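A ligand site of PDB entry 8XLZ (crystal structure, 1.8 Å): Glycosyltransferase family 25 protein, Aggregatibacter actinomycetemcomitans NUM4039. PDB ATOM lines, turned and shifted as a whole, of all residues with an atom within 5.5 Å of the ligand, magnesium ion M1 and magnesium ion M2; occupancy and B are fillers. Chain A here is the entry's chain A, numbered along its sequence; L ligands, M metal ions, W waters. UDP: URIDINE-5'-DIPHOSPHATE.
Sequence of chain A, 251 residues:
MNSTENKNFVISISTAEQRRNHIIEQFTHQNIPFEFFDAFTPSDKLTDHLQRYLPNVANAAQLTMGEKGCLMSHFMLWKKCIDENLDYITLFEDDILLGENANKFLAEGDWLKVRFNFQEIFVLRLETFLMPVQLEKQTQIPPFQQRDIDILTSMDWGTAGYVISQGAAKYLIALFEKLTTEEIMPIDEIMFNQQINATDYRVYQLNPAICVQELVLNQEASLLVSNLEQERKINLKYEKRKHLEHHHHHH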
ATOM      1  N   ILE A  11     -14.452   4.522 -21.063  1.00  0.00           N
ATOM      2  CA  ILE A  11     -13.775   3.356 -20.526  1.00  0.00           C
ATOM      3  C   ILE A  11     -12.755   3.815 -19.485  1.00  0.00           C
ATOM      4  O   ILE A  11     -11.878   4.613 -19.803  1.00  0.00           O
ATOM      5  CB  ILE A  11     -13.045   2.593 -21.650  1.00  0.00           C
ATOM      6  CG1 ILE A  11     -14.051   2.080 -22.665  1.00  0.00           C
ATOM      7  CG2 ILE A  11     -12.203   1.455 -21.071  1.00  0.00           C
ATOM      8  CD1 ILE A  11     -13.452   1.701 -23.995  1.00  0.00           C
ATOM      9  N   SER A  12     -12.877   3.331 -18.253  1.00  0.00           N
ATOM     10  CA  SER A  12     -12.081   3.843 -17.148  1.00  0.00           C
ATOM     11  C   SER A  12     -11.968   2.810 -16.044  1.00  0.00           C
ATOM     12  O   SER A  12     -12.954   2.211 -15.644  1.00  0.00           O
ATOM     13  CB  SER A  12     -12.731   5.092 -16.574  1.00  0.00           C
ATOM     14  OG  SER A  12     -11.912   5.706 -15.592  1.00  0.00           O
ATOM     15  N   ILE A  13     -10.756   2.577 -15.565  1.00  0.00           N
ATOM     16  CA  ILE A  13     -10.542   1.659 -14.460  1.00  0.00           C
ATOM     17  C   ILE A  13     -11.308   2.223 -13.248  1.00  0.00           C
ATOM     18  O   ILE A  13     -11.224   3.424 -12.980  1.00  0.00           O
ATOM     19  CB  ILE A  13      -9.040   1.461 -14.164  1.00  0.00           C
ATOM     20  CG1 ILE A  13      -8.385   0.727 -15.345  1.00  0.00           C
ATOM     21  CG2 ILE A  13      -8.821   0.682 -12.878  1.00  0.00           C
ATOM     22  CD1 ILE A  13      -6.873   0.630 -15.247  1.00  0.00           C
ATOM     23  N   ARG A  19      -8.191  10.446 -13.185  1.00  0.00           N
ATOM     24  CA  ARG A  19      -8.739  10.467 -14.544  1.00  0.00           C
ATOM     25  C   ARG A  19     -10.264  10.675 -14.520  1.00  0.00           C
ATOM     26  O   ARG A  19     -10.778  11.472 -15.300  1.00  0.00           O
ATOM     27  CB  ARG A  19      -8.399   9.176 -15.281  1.00  0.00           C
ATOM     28  CG  ARG A  19      -6.936   9.026 -15.636  1.00  0.00           C
ATOM     29  CD  ARG A  19      -6.750   7.805 -16.505  1.00  0.00           C
ATOM     30  NE  ARG A  19      -5.427   7.756 -17.112  1.00  0.00           N
ATOM     31  CZ  ARG A  19      -5.085   6.999 -18.136  1.00  0.00           C
ATOM     32  NH1 ARG A  19      -3.847   7.048 -18.602  1.00  0.00           N
ATOM     33  NH2 ARG A  19      -5.973   6.197 -18.714  1.00  0.00           N
ATOM     34  N   ALA A  39     -13.469  -0.453 -16.777  1.00  0.00           N
ATOM     35  CA  ALA A  39     -12.521  -1.135 -17.626  1.00  0.00           C
ATOM     36  C   ALA A  39     -12.121  -2.487 -17.049  1.00  0.00           C
ATOM     37  O   ALA A  39     -12.005  -2.648 -15.833  1.00  0.00           O
ATOM     38  CB  ALA A  39     -11.286  -0.271 -17.824  1.00  0.00           C
ATOM     39  N   PHE A  40     -11.905  -3.445 -17.922  1.00  0.00           N
ATOM     40  CA  PHE A  40     -11.318  -4.725 -17.520  1.00  0.00           C
ATOM     41  C   PHE A  40      -9.840  -4.530 -17.271  1.00  0.00           C
ATOM     42  O   PHE A  40      -9.140  -3.919 -18.083  1.00  0.00           O
ATOM     43  CB  PHE A  40     -11.505  -5.768 -18.615  1.00  0.00           C
ATOM     44  CG  PHE A  40     -12.916  -6.195 -18.784  1.00  0.00           C
ATOM     45  CD1 PHE A  40     -13.778  -5.485 -19.600  1.00  0.00           C
ATOM     46  CD2 PHE A  40     -13.397  -7.299 -18.097  1.00  0.00           C
ATOM     47  CE1 PHE A  40     -15.097  -5.894 -19.733  1.00  0.00           C
ATOM     48  CE2 PHE A  40     -14.712  -7.706 -18.213  1.00  0.00           C
ATOM     49  CZ  PHE A  40     -15.555  -6.998 -19.051  1.00  0.00           C
ATOM     50  N   THR A  41      -9.348  -5.067 -16.156  1.00  0.00           N
ATOM     51  CA  THR A  41      -7.912  -5.012 -15.811  1.00  0.00           C
ATOM     52  C   THR A  41      -7.399  -6.425 -15.581  1.00  0.00           C
ATOM     53  O   THR A  41      -8.184  -7.375 -15.518  1.00  0.00           O
ATOM     54  CB  THR A  41      -7.680  -4.146 -14.566  1.00  0.00           C
ATOM     55  OG1 THR A  41      -8.360  -4.721 -13.465  1.00  0.00           O
ATOM     56  CG2 THR A  41      -8.219  -2.730 -14.761  1.00  0.00           C
ATOM     57  N   PRO A  42      -6.079  -6.595 -15.478  1.00  0.00           N
ATOM     58  CA  PRO A  42      -5.577  -7.963 -15.226  1.00  0.00           C
ATOM     59  C   PRO A  42      -6.151  -8.473 -13.918  1.00  0.00           C
ATOM     60  O   PRO A  42      -5.960  -7.856 -12.882  1.00  0.00           O
ATOM     61  CB  PRO A  42      -4.064  -7.779 -15.168  1.00  0.00           C
ATOM     62  CG  PRO A  42      -3.811  -6.508 -15.928  1.00  0.00           C
ATOM     63  CD  PRO A  42      -4.986  -5.624 -15.661  1.00  0.00           C
ATOM     64  N   MET A  65      -1.469  -8.185 -20.755  1.00  0.00           N
ATOM     65  CA  MET A  65      -2.760  -8.400 -20.164  1.00  0.00           C
ATOM     66  C   MET A  65      -3.541  -7.080 -20.073  1.00  0.00           C
ATOM     67  O   MET A  65      -4.756  -7.055 -20.227  1.00  0.00           O
ATOM     68  CB  MET A  65      -2.629  -9.043 -18.789  1.00  0.00           C
ATOM     69  CG  MET A  65      -3.930  -9.629 -18.282  1.00  0.00           C
ATOM     70  SD  MET A  65      -4.651 -10.921 -19.306  1.00  0.00           S
ATOM     71  CE  MET A  65      -3.291 -12.062 -19.542  1.00  0.00           C
ATOM     72  N   GLY A  66      -2.819  -5.992 -19.814  1.00  0.00           N
ATOM     73  CA  GLY A  66      -3.425  -4.669 -19.782  1.00  0.00           C
ATOM     74  C   GLY A  66      -4.041  -4.292 -21.126  1.00  0.00           C
ATOM     75  O   GLY A  66      -5.142  -3.709 -21.184  1.00  0.00           O
ATOM     76  N   GLU A  67      -3.322  -4.610 -22.204  1.00  0.00           N
ATOM     77  CA  GLU A  67      -3.828  -4.372 -23.535  1.00  0.00           C
ATOM     78  C   GLU A  67      -5.039  -5.256 -23.817  1.00  0.00           C
ATOM     79  O   GLU A  67      -5.976  -4.839 -24.491  1.00  0.00           O
ATOM     80  CB  GLU A  67      -2.743  -4.611 -24.592  1.00  0.00           C
ATOM     81  CG  GLU A  67      -1.720  -3.492 -24.625  1.00  0.00           C
ATOM     82  CD  GLU A  67      -0.409  -3.852 -25.292  1.00  0.00           C
ATOM     83  OE1 GLU A  67       0.414  -2.941 -25.389  1.00  0.00           O
ATOM     84  OE2 GLU A  67      -0.138  -5.034 -25.638  1.00  0.00           O
ATOM     85  N   GLY A  69      -7.100  -6.182 -21.543  1.00  0.00           N
ATOM     86  CA  GLY A  69      -8.163  -5.559 -20.774  1.00  0.00           C
ATOM     87  C   GLY A  69      -8.824  -4.400 -21.534  1.00  0.00           C
ATOM     88  O   GLY A  69     -10.059  -4.286 -21.573  1.00  0.00           O
ATOM     89  N   CYS A  70      -8.005  -3.546 -22.142  1.00  0.00           N
ATOM     90  CA  CYS A  70      -8.520  -2.448 -22.958  1.00  0.00           C
ATOM     91  C   CYS A  70      -9.350  -2.996 -24.135  1.00  0.00           C
ATOM     92  O   CYS A  70     -10.475  -2.578 -24.349  1.00  0.00           O
ATOM     93  CB  CYS A  70      -7.355  -1.586 -23.462  1.00  0.00           C
ATOM     94  SG  CYS A  70      -7.904  -0.195 -24.473  1.00  0.00           S
ATOM     95  N   LEU A  71      -8.802  -3.989 -24.837  1.00  0.00           N
ATOM     96  CA  LEU A  71      -9.528  -4.674 -25.904  1.00  0.00           C
ATOM     97  C   LEU A  71     -10.892  -5.229 -25.434  1.00  0.00           C
ATOM     98  O   LEU A  71     -11.914  -5.054 -26.106  1.00  0.00           O
ATOM     99  CB  LEU A  71      -8.672  -5.822 -26.494  1.00  0.00           C
ATOM    100  CG  LEU A  71      -9.418  -6.849 -27.361  1.00  0.00           C
ATOM    101  CD1 LEU A  71     -10.169  -6.207 -28.517  1.00  0.00           C
ATOM    102  CD2 LEU A  71      -8.461  -7.893 -27.919  1.00  0.00           C
ATOM    103  N   SER A  73     -12.690  -4.301 -22.994  1.00  0.00           N
ATOM    104  CA  SER A  73     -13.581  -3.190 -22.631  1.00  0.00           C
ATOM    105  C   SER A  73     -14.310  -2.649 -23.883  1.00  0.00           C
ATOM    106  O   SER A  73     -15.518  -2.517 -23.882  1.00  0.00           O
ATOM    107  CB  SER A  73     -12.805  -2.093 -21.927  1.00  0.00           C
ATOM    108  OG  SER A  73     -12.146  -2.632 -20.796  1.00  0.00           O
ATOM    109  N   PHE A  92     -15.114   6.530 -25.575  1.00  0.00           N
ATOM    110  CA  PHE A  92     -13.928   7.275 -25.191  1.00  0.00           C
ATOM    111  C   PHE A  92     -13.078   6.487 -24.227  1.00  0.00           C
ATOM    112  O   PHE A  92     -13.561   5.589 -23.536  1.00  0.00           O
ATOM    113  CB  PHE A  92     -14.313   8.574 -24.504  1.00  0.00           C
ATOM    114  CG  PHE A  92     -15.125   9.493 -25.365  1.00  0.00           C
ATOM    115  CD1 PHE A  92     -14.497  10.353 -26.245  1.00  0.00           C
ATOM    116  CD2 PHE A  92     -16.510   9.465 -25.308  1.00  0.00           C
ATOM    117  CE1 PHE A  92     -15.239  11.179 -27.053  1.00  0.00           C
ATOM    118  CE2 PHE A  92     -17.262  10.305 -26.121  1.00  0.00           C
ATOM    119  CZ  PHE A  92     -16.625  11.151 -26.996  1.00  0.00           C
ATOM    120  N   GLU A  93     -11.799   6.851 -24.175  1.00  0.00           N
ATOM    121  CA  GLU A  93     -10.907   6.369 -23.145  1.00  0.00           C
ATOM    122  C   GLU A  93     -10.684   7.501 -22.152  1.00  0.00           C
ATOM    123  O   GLU A  93     -10.896   8.695 -22.482  1.00  0.00           O
ATOM    124  CB  GLU A  93      -9.614   5.827 -23.772  1.00  0.00           C
ATOM    125  CG  GLU A  93      -9.802   4.471 -24.453  1.00  0.00           C
ATOM    126  CD  GLU A  93      -8.630   4.017 -25.323  1.00  0.00           C
ATOM    127  OE1 GLU A  93      -8.685   2.893 -25.832  1.00  0.00           O
ATOM    128  OE2 GLU A  93      -7.681   4.778 -25.522  1.00  0.00           O
ATOM    129  N   ASP A  94     -10.315   7.146 -20.920  1.00  0.00           N
ATOM    130  CA  ASP A  94     -10.492   8.105 -19.823  1.00  0.00           C
ATOM    131  C   ASP A  94      -9.360   9.122 -19.686  1.00  0.00           C
ATOM    132  O   ASP A  94      -9.277   9.806 -18.686  1.00  0.00           O
ATOM    133  CB  ASP A  94     -10.801   7.422 -18.504  1.00  0.00           C
ATOM    134  CG  ASP A  94      -9.653   6.602 -17.974  1.00  0.00           C
ATOM    135  OD1 ASP A  94      -8.693   6.391 -18.731  1.00  0.00           O
ATOM    136  OD2 ASP A  94      -9.726   6.186 -16.790  1.00  0.00           O
ATOM    137  N   ASP A  95      -8.505   9.211 -20.700  1.00  0.00           N
ATOM    138  CA  ASP A  95      -7.524  10.265 -20.753  1.00  0.00           C
ATOM    139  C   ASP A  95      -7.790  11.340 -21.832  1.00  0.00           C
ATOM    140  O   ASP A  95      -6.880  12.137 -22.098  1.00  0.00           O
ATOM    141  CB  ASP A  95      -6.145   9.632 -20.943  1.00  0.00           C
ATOM    142  CG  ASP A  95      -5.997   8.904 -22.289  1.00  0.00           C
ATOM    143  OD1 ASP A  95      -7.009   8.690 -23.012  1.00  0.00           O
ATOM    144  OD2 ASP A  95      -4.856   8.576 -22.599  1.00  0.00           O
ATOM    145  N   ASP A 156       0.942   2.859 -30.170  1.00  0.00           N
ATOM    146  CA  ASP A 156      -0.311   2.489 -30.786  1.00  0.00           C
ATOM    147  C   ASP A 156      -1.065   3.771 -31.150  1.00  0.00           C
ATOM    148  O   ASP A 156      -1.015   4.774 -30.431  1.00  0.00           O
ATOM    149  CB  ASP A 156      -1.159   1.670 -29.824  1.00  0.00           C
ATOM    150  CG  ASP A 156      -0.564   0.293 -29.533  1.00  0.00           C
ATOM    151  OD1 ASP A 156      -0.027  -0.388 -30.461  1.00  0.00           O
ATOM    152  OD2 ASP A 156      -0.670  -0.109 -28.348  1.00  0.00           O
ATOM    153  N   TRP A 157      -1.772   3.745 -32.248  1.00  0.00           N
ATOM    154  CA  TRP A 157      -2.638   4.872 -32.582  1.00  0.00           C
ATOM    155  C   TRP A 157      -3.853   4.869 -31.650  1.00  0.00           C
ATOM    156  O   TRP A 157      -4.214   3.834 -31.080  1.00  0.00           O
ATOM    157  CB  TRP A 157      -3.083   4.780 -34.019  1.00  0.00           C
ATOM    158  CG  TRP A 157      -3.495   6.074 -34.664  1.00  0.00           C
ATOM    159  CD1 TRP A 157      -2.970   7.332 -34.449  1.00  0.00           C
ATOM    160  CD2 TRP A 157      -4.465   6.228 -35.696  1.00  0.00           C
ATOM    161  NE1 TRP A 157      -3.579   8.250 -35.279  1.00  0.00           N
ATOM    162  CE2 TRP A 157      -4.484   7.591 -36.070  1.00  0.00           C
ATOM    163  CE3 TRP A 157      -5.312   5.340 -36.364  1.00  0.00           C
ATOM    164  CZ2 TRP A 157      -5.332   8.092 -37.053  1.00  0.00           C
ATOM    165  CZ3 TRP A 157      -6.159   5.827 -37.346  1.00  0.00           C
ATOM    166  CH2 TRP A 157      -6.146   7.193 -37.691  1.00  0.00           C
ATOM    167  N   GLY A 158      -4.477   6.038 -31.526  1.00  0.00           N
ATOM    168  CA  GLY A 158      -5.542   6.254 -30.567  1.00  0.00           C
ATOM    169  C   GLY A 158      -6.836   5.511 -30.850  1.00  0.00           C
ATOM    170  O   GLY A 158      -7.232   5.363 -32.000  1.00  0.00           O
ATOM    171  N   THR A 159      -7.454   5.005 -29.776  1.00  0.00           N
ATOM    172  CA  THR A 159      -8.809   4.451 -29.802  1.00  0.00           C
ATOM    173  C   THR A 159      -9.566   5.118 -28.704  1.00  0.00           C
ATOM    174  O   THR A 159     -10.407   4.508 -27.997  1.00  0.00           O
ATOM    175  CB  THR A 159      -8.845   2.905 -29.611  1.00  0.00           C
ATOM    176  OG1 THR A 159      -8.074   2.531 -28.487  1.00  0.00           O
ATOM    177  CG2 THR A 159      -8.341   2.197 -30.880  1.00  0.00           C
ATOM    178  N   ALA A 160      -9.271   6.410 -28.541  1.00  0.00           N
ATOM    179  CA  ALA A 160      -9.696   7.167 -27.366  1.00  0.00           C
ATOM    180  C   ALA A 160     -10.953   7.958 -27.601  1.00  0.00           C
ATOM    181  O   ALA A 160     -11.493   8.514 -26.648  1.00  0.00           O
ATOM    182  CB  ALA A 160      -8.575   8.108 -26.927  1.00  0.00           C
ATOM    183  N   GLN A 213      -5.930  12.902 -26.762  1.00  0.00           N
ATOM    184  CA  GLN A 213      -5.437  12.292 -25.532  1.00  0.00           C
ATOM    185  C   GLN A 213      -4.508  13.250 -24.813  1.00  0.00           C
ATOM    186  O   GLN A 213      -3.740  13.957 -25.460  1.00  0.00           O
ATOM    187  CB  GLN A 213      -4.683  11.015 -25.829  1.00  0.00           C
ATOM    188  CG  GLN A 213      -5.538   9.921 -26.420  1.00  0.00           C
ATOM    189  CD  GLN A 213      -4.705   8.703 -26.706  1.00  0.00           C
ATOM    190  OE1 GLN A 213      -3.973   8.266 -25.846  1.00  0.00           O
ATOM    191  NE2 GLN A 213      -4.811   8.163 -27.906  1.00  0.00           N
HETATM  192  N1  UDP L   1      -7.293   0.326 -19.750  1.00  0.00           N
HETATM  193  C2  UDP L   1      -7.994  -0.920 -19.670  1.00  0.00           C
HETATM  194  N3  UDP L   1      -7.437  -1.925 -18.992  1.00  0.00           N
HETATM  195  C4  UDP L   1      -6.243  -1.805 -18.384  1.00  0.00           C
HETATM  196  C5  UDP L   1      -5.504  -0.617 -18.473  1.00  0.00           C
HETATM  197  C6  UDP L   1      -6.064   0.457 -19.175  1.00  0.00           C
HETATM  198  O2  UDP L   1      -9.112  -1.096 -20.218  1.00  0.00           O
HETATM  199  O4  UDP L   1      -5.805  -2.782 -17.765  1.00  0.00           O
HETATM  200  C1' UDP L   1      -7.893   1.430 -20.494  1.00  0.00           C
HETATM  201  C2' UDP L   1      -7.898   2.724 -19.703  1.00  0.00           C
HETATM  202  O2' UDP L   1      -8.961   2.714 -18.721  1.00  0.00           O
HETATM  203  C3' UDP L   1      -8.098   3.735 -20.803  1.00  0.00           C
HETATM  204  C4' UDP L   1      -7.456   3.080 -22.043  1.00  0.00           C
HETATM  205  O4' UDP L   1      -7.167   1.719 -21.695  1.00  0.00           O
HETATM  206  O3' UDP L   1      -9.506   3.933 -21.037  1.00  0.00           O
HETATM  207  C5' UDP L   1      -6.206   3.806 -22.498  1.00  0.00           C
HETATM  208  O5' UDP L   1      -5.210   3.771 -21.490  1.00  0.00           O
HETATM  209  PA  UDP L   1      -3.861   4.650 -21.704  1.00  0.00           P
HETATM  210  O1A UDP L   1      -3.110   4.419 -20.417  1.00  0.00           O
HETATM  211  O2A UDP L   1      -4.298   6.042 -22.146  1.00  0.00           O
HETATM  212  O3A UDP L   1      -2.976   3.931 -22.844  1.00  0.00           O
HETATM  213  PB  UDP L   1      -2.761   4.209 -24.433  1.00  0.00           P
HETATM  214  O1B UDP L   1      -1.257   4.436 -24.437  1.00  0.00           O
HETATM  215  O2B UDP L   1      -3.556   5.346 -24.969  1.00  0.00           O
HETATM  216  O3B UDP L   1      -3.163   2.938 -25.157  1.00  0.00           O
HETATM  217 MG    MG M   1      -4.156   7.145 -24.011  1.00  0.00          MG
HETATM  218 MG    MG M   2      -4.446   2.871 -26.929  1.00  0.00          MG
HETATM  219  O   HOH W   1      -3.364   1.000 -27.180  1.00  0.00           O
HETATM  220  O   HOH W   2      -2.809   3.874 -27.941  1.00  0.00           O
HETATM  221  O   HOH W   3      -6.226   6.735 -24.556  1.00  0.00           O
HETATM  222  O   HOH W   4      -5.285   2.293 -28.844  1.00  0.00           O
HETATM  223  O   HOH W   5      -2.184   7.831 -23.395  1.00  0.00           O
HETATM  224  O   HOH W   6      -8.423   3.984 -16.534  1.00  0.00           O
HETATM  225  O   HOH W   7      -1.399   7.244 -26.841  1.00  0.00           O
HETATM  226  O   HOH W   8      -3.872  -2.387 -15.855  1.00  0.00           O
HETATM  227  O   HOH W   9      -6.056   1.961 -25.783  1.00  0.00           O
HETATM  228  O   HOH W  10      -5.599   4.709 -27.080  1.00  0.00           O
HETATM  229  O   HOH W  11      -0.359   4.079 -27.082  1.00  0.00           O
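The backbone carbonyl oxygen (O) of Ile 11 sits at hydrogen-bond distance from an oxygen (O3') of the ligand, at 2.8 Å. A nitrogen (N3) of the ligand is in hydrogen-bond range of the backbone carbonyl oxygen (O) of Phe 40 (2.8 Å). An oxygen (O2) of the ligand sits close to the backbone NH (N) of Cys 70 (3.3 Å). O4' of the ligand lies within hydrogen-bond range of SG of Cys 70 (3.5 Å). The guanidinium group (NH1) of Arg 19 is in salt-bridge range of an oxygen (O1A) of the ligand, 3.3 Å away. The backbone NH (N) of Asp 94 is in hydrogen-bond range of an oxygen (O3') of the ligand, 3.3 Å away. The side-chain carboxylate (OD1) of Asp 94 lies close to an oxygen (O3') of the ligand (3.5 Å). OG of Ser 73 lies within hydrogen-bond range of O2 of the ligand.
The backbone carbonyl oxygen (O) of Ile 11 is in hydrogen-bond range of the backbone NH (N) of Asp 94 (3.2 Å). The backbone carbonyl oxygen of Phe 92 is in hydrogen-bond range of the backbone NH of Ile 11 (2.8 Å). N of Phe 40 sits at hydrogen-bond distance from OG of Ser 73. The guanidinium group of Arg 19 is in salt-bridge range of the side-chain carboxylate of Asp 94. The side-chain hydroxyl of Ser 12 lies within hydrogen-bond range of the side-chain carboxylate of Asp 94 (2.5 Å). The backbone carbonyl oxygen of Ala 160 is in hydrogen-bond range of the backbone NH of Glu 93, 3.0 Å away. The backbone NH (N) of Ala 39 is in hydrogen-bond range of the backbone carbonyl oxygen (O) of Ser 12 (2.9 Å). The backbone carbonyl oxygen (O) of Gly 69 sits at hydrogen-bond distance from the side-chain hydroxyl (OG) of Ser 73, at 2.8 Å.
Ser 12 touches the ligand. N of Ile 13 touches O2' of the ligand, 3.6 Å away. Ala 39 touches the ligand (CB to O2, 3.3 Å). CA of Thr 41 touches O4 of the ligand (3.6 Å). CD of Pro 42 touches O4 of the ligand, 3.6 Å away. O of Gly 66 touches C4 of the ligand, 3.6 Å away. Gly 69 touches the ligand (C to O2, 3.6 Å). Glu 93 touches the ligand (CB to O3', 3.3 Å). Hydrophobic or aromatic side chains that line the ligand: Ile 11, Ile 13, Ala 39 and Pro 42. Of the 25 residues printed, 16 come within 4 Å of the ligand. The nearest printed residue that does not touch the ligand is Met 65 (5.0 Å).
Of the 25 residues printed, 2 come within 4 Å of magnesium ion M1.
Thr 159 touches magnesium ion M2 (OG1 to MG, 3.96 Å). Of the 25 residues printed, 1 comes within 4 Å of magnesium ion M2.
Magnesium ion M1 is bound by an oxygen (O2B) of the ligand, the side-chain carboxylate of Asp 95, the side-chain amide oxygen of Gln 213, an oxygen (O2A) of the ligand, water W5 and water W3.
Water W4 is bound to magnesium ion M2, 2.2 Å away. Magnesium ion M2 is bound by water W2. Water W10 binds magnesium ion M2 (2.2 Å). Water W9 binds magnesium ion M2 (2.2 Å). Magnesium ion M2 is bound by water W1, at 2.2 Å. O3B of the ligand binds magnesium ion M2. Magnesium ion M2 has six donor atoms within binding distance.
Water W3 lies within hydrogen-bond range of the side-chain carboxylate (OD1) of Asp 95 (2.6 Å) and the side-chain carboxylate (OE2) of Glu 93 (2.6 Å). Water W9 lies within hydrogen-bond range of the side-chain carboxylate of Glu 93 (2.8 Å), the side-chain sulfur of Cys 70 (3.1 Å) and the side-chain hydroxyl of Thr 159 (3.4 Å). Water W10 bridges the side-chain carboxylate of Glu 93 and the backbone NH of Thr 159. Water W4 bridges OG1 of Thr 159 (2.8 Å) and O of Trp 157 (2.9 Å). Water W6 lies within hydrogen-bond range of OD2 of Asp 94 (2.6 Å), O2' of the ligand (2.6 Å) and N of Ile 13 (2.9 Å). Water W11 lies within hydrogen-bond range of an oxygen (O1B) of the ligand (2.8 Å) and the backbone carbonyl oxygen (O) of Asp 156 (3.5 Å).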
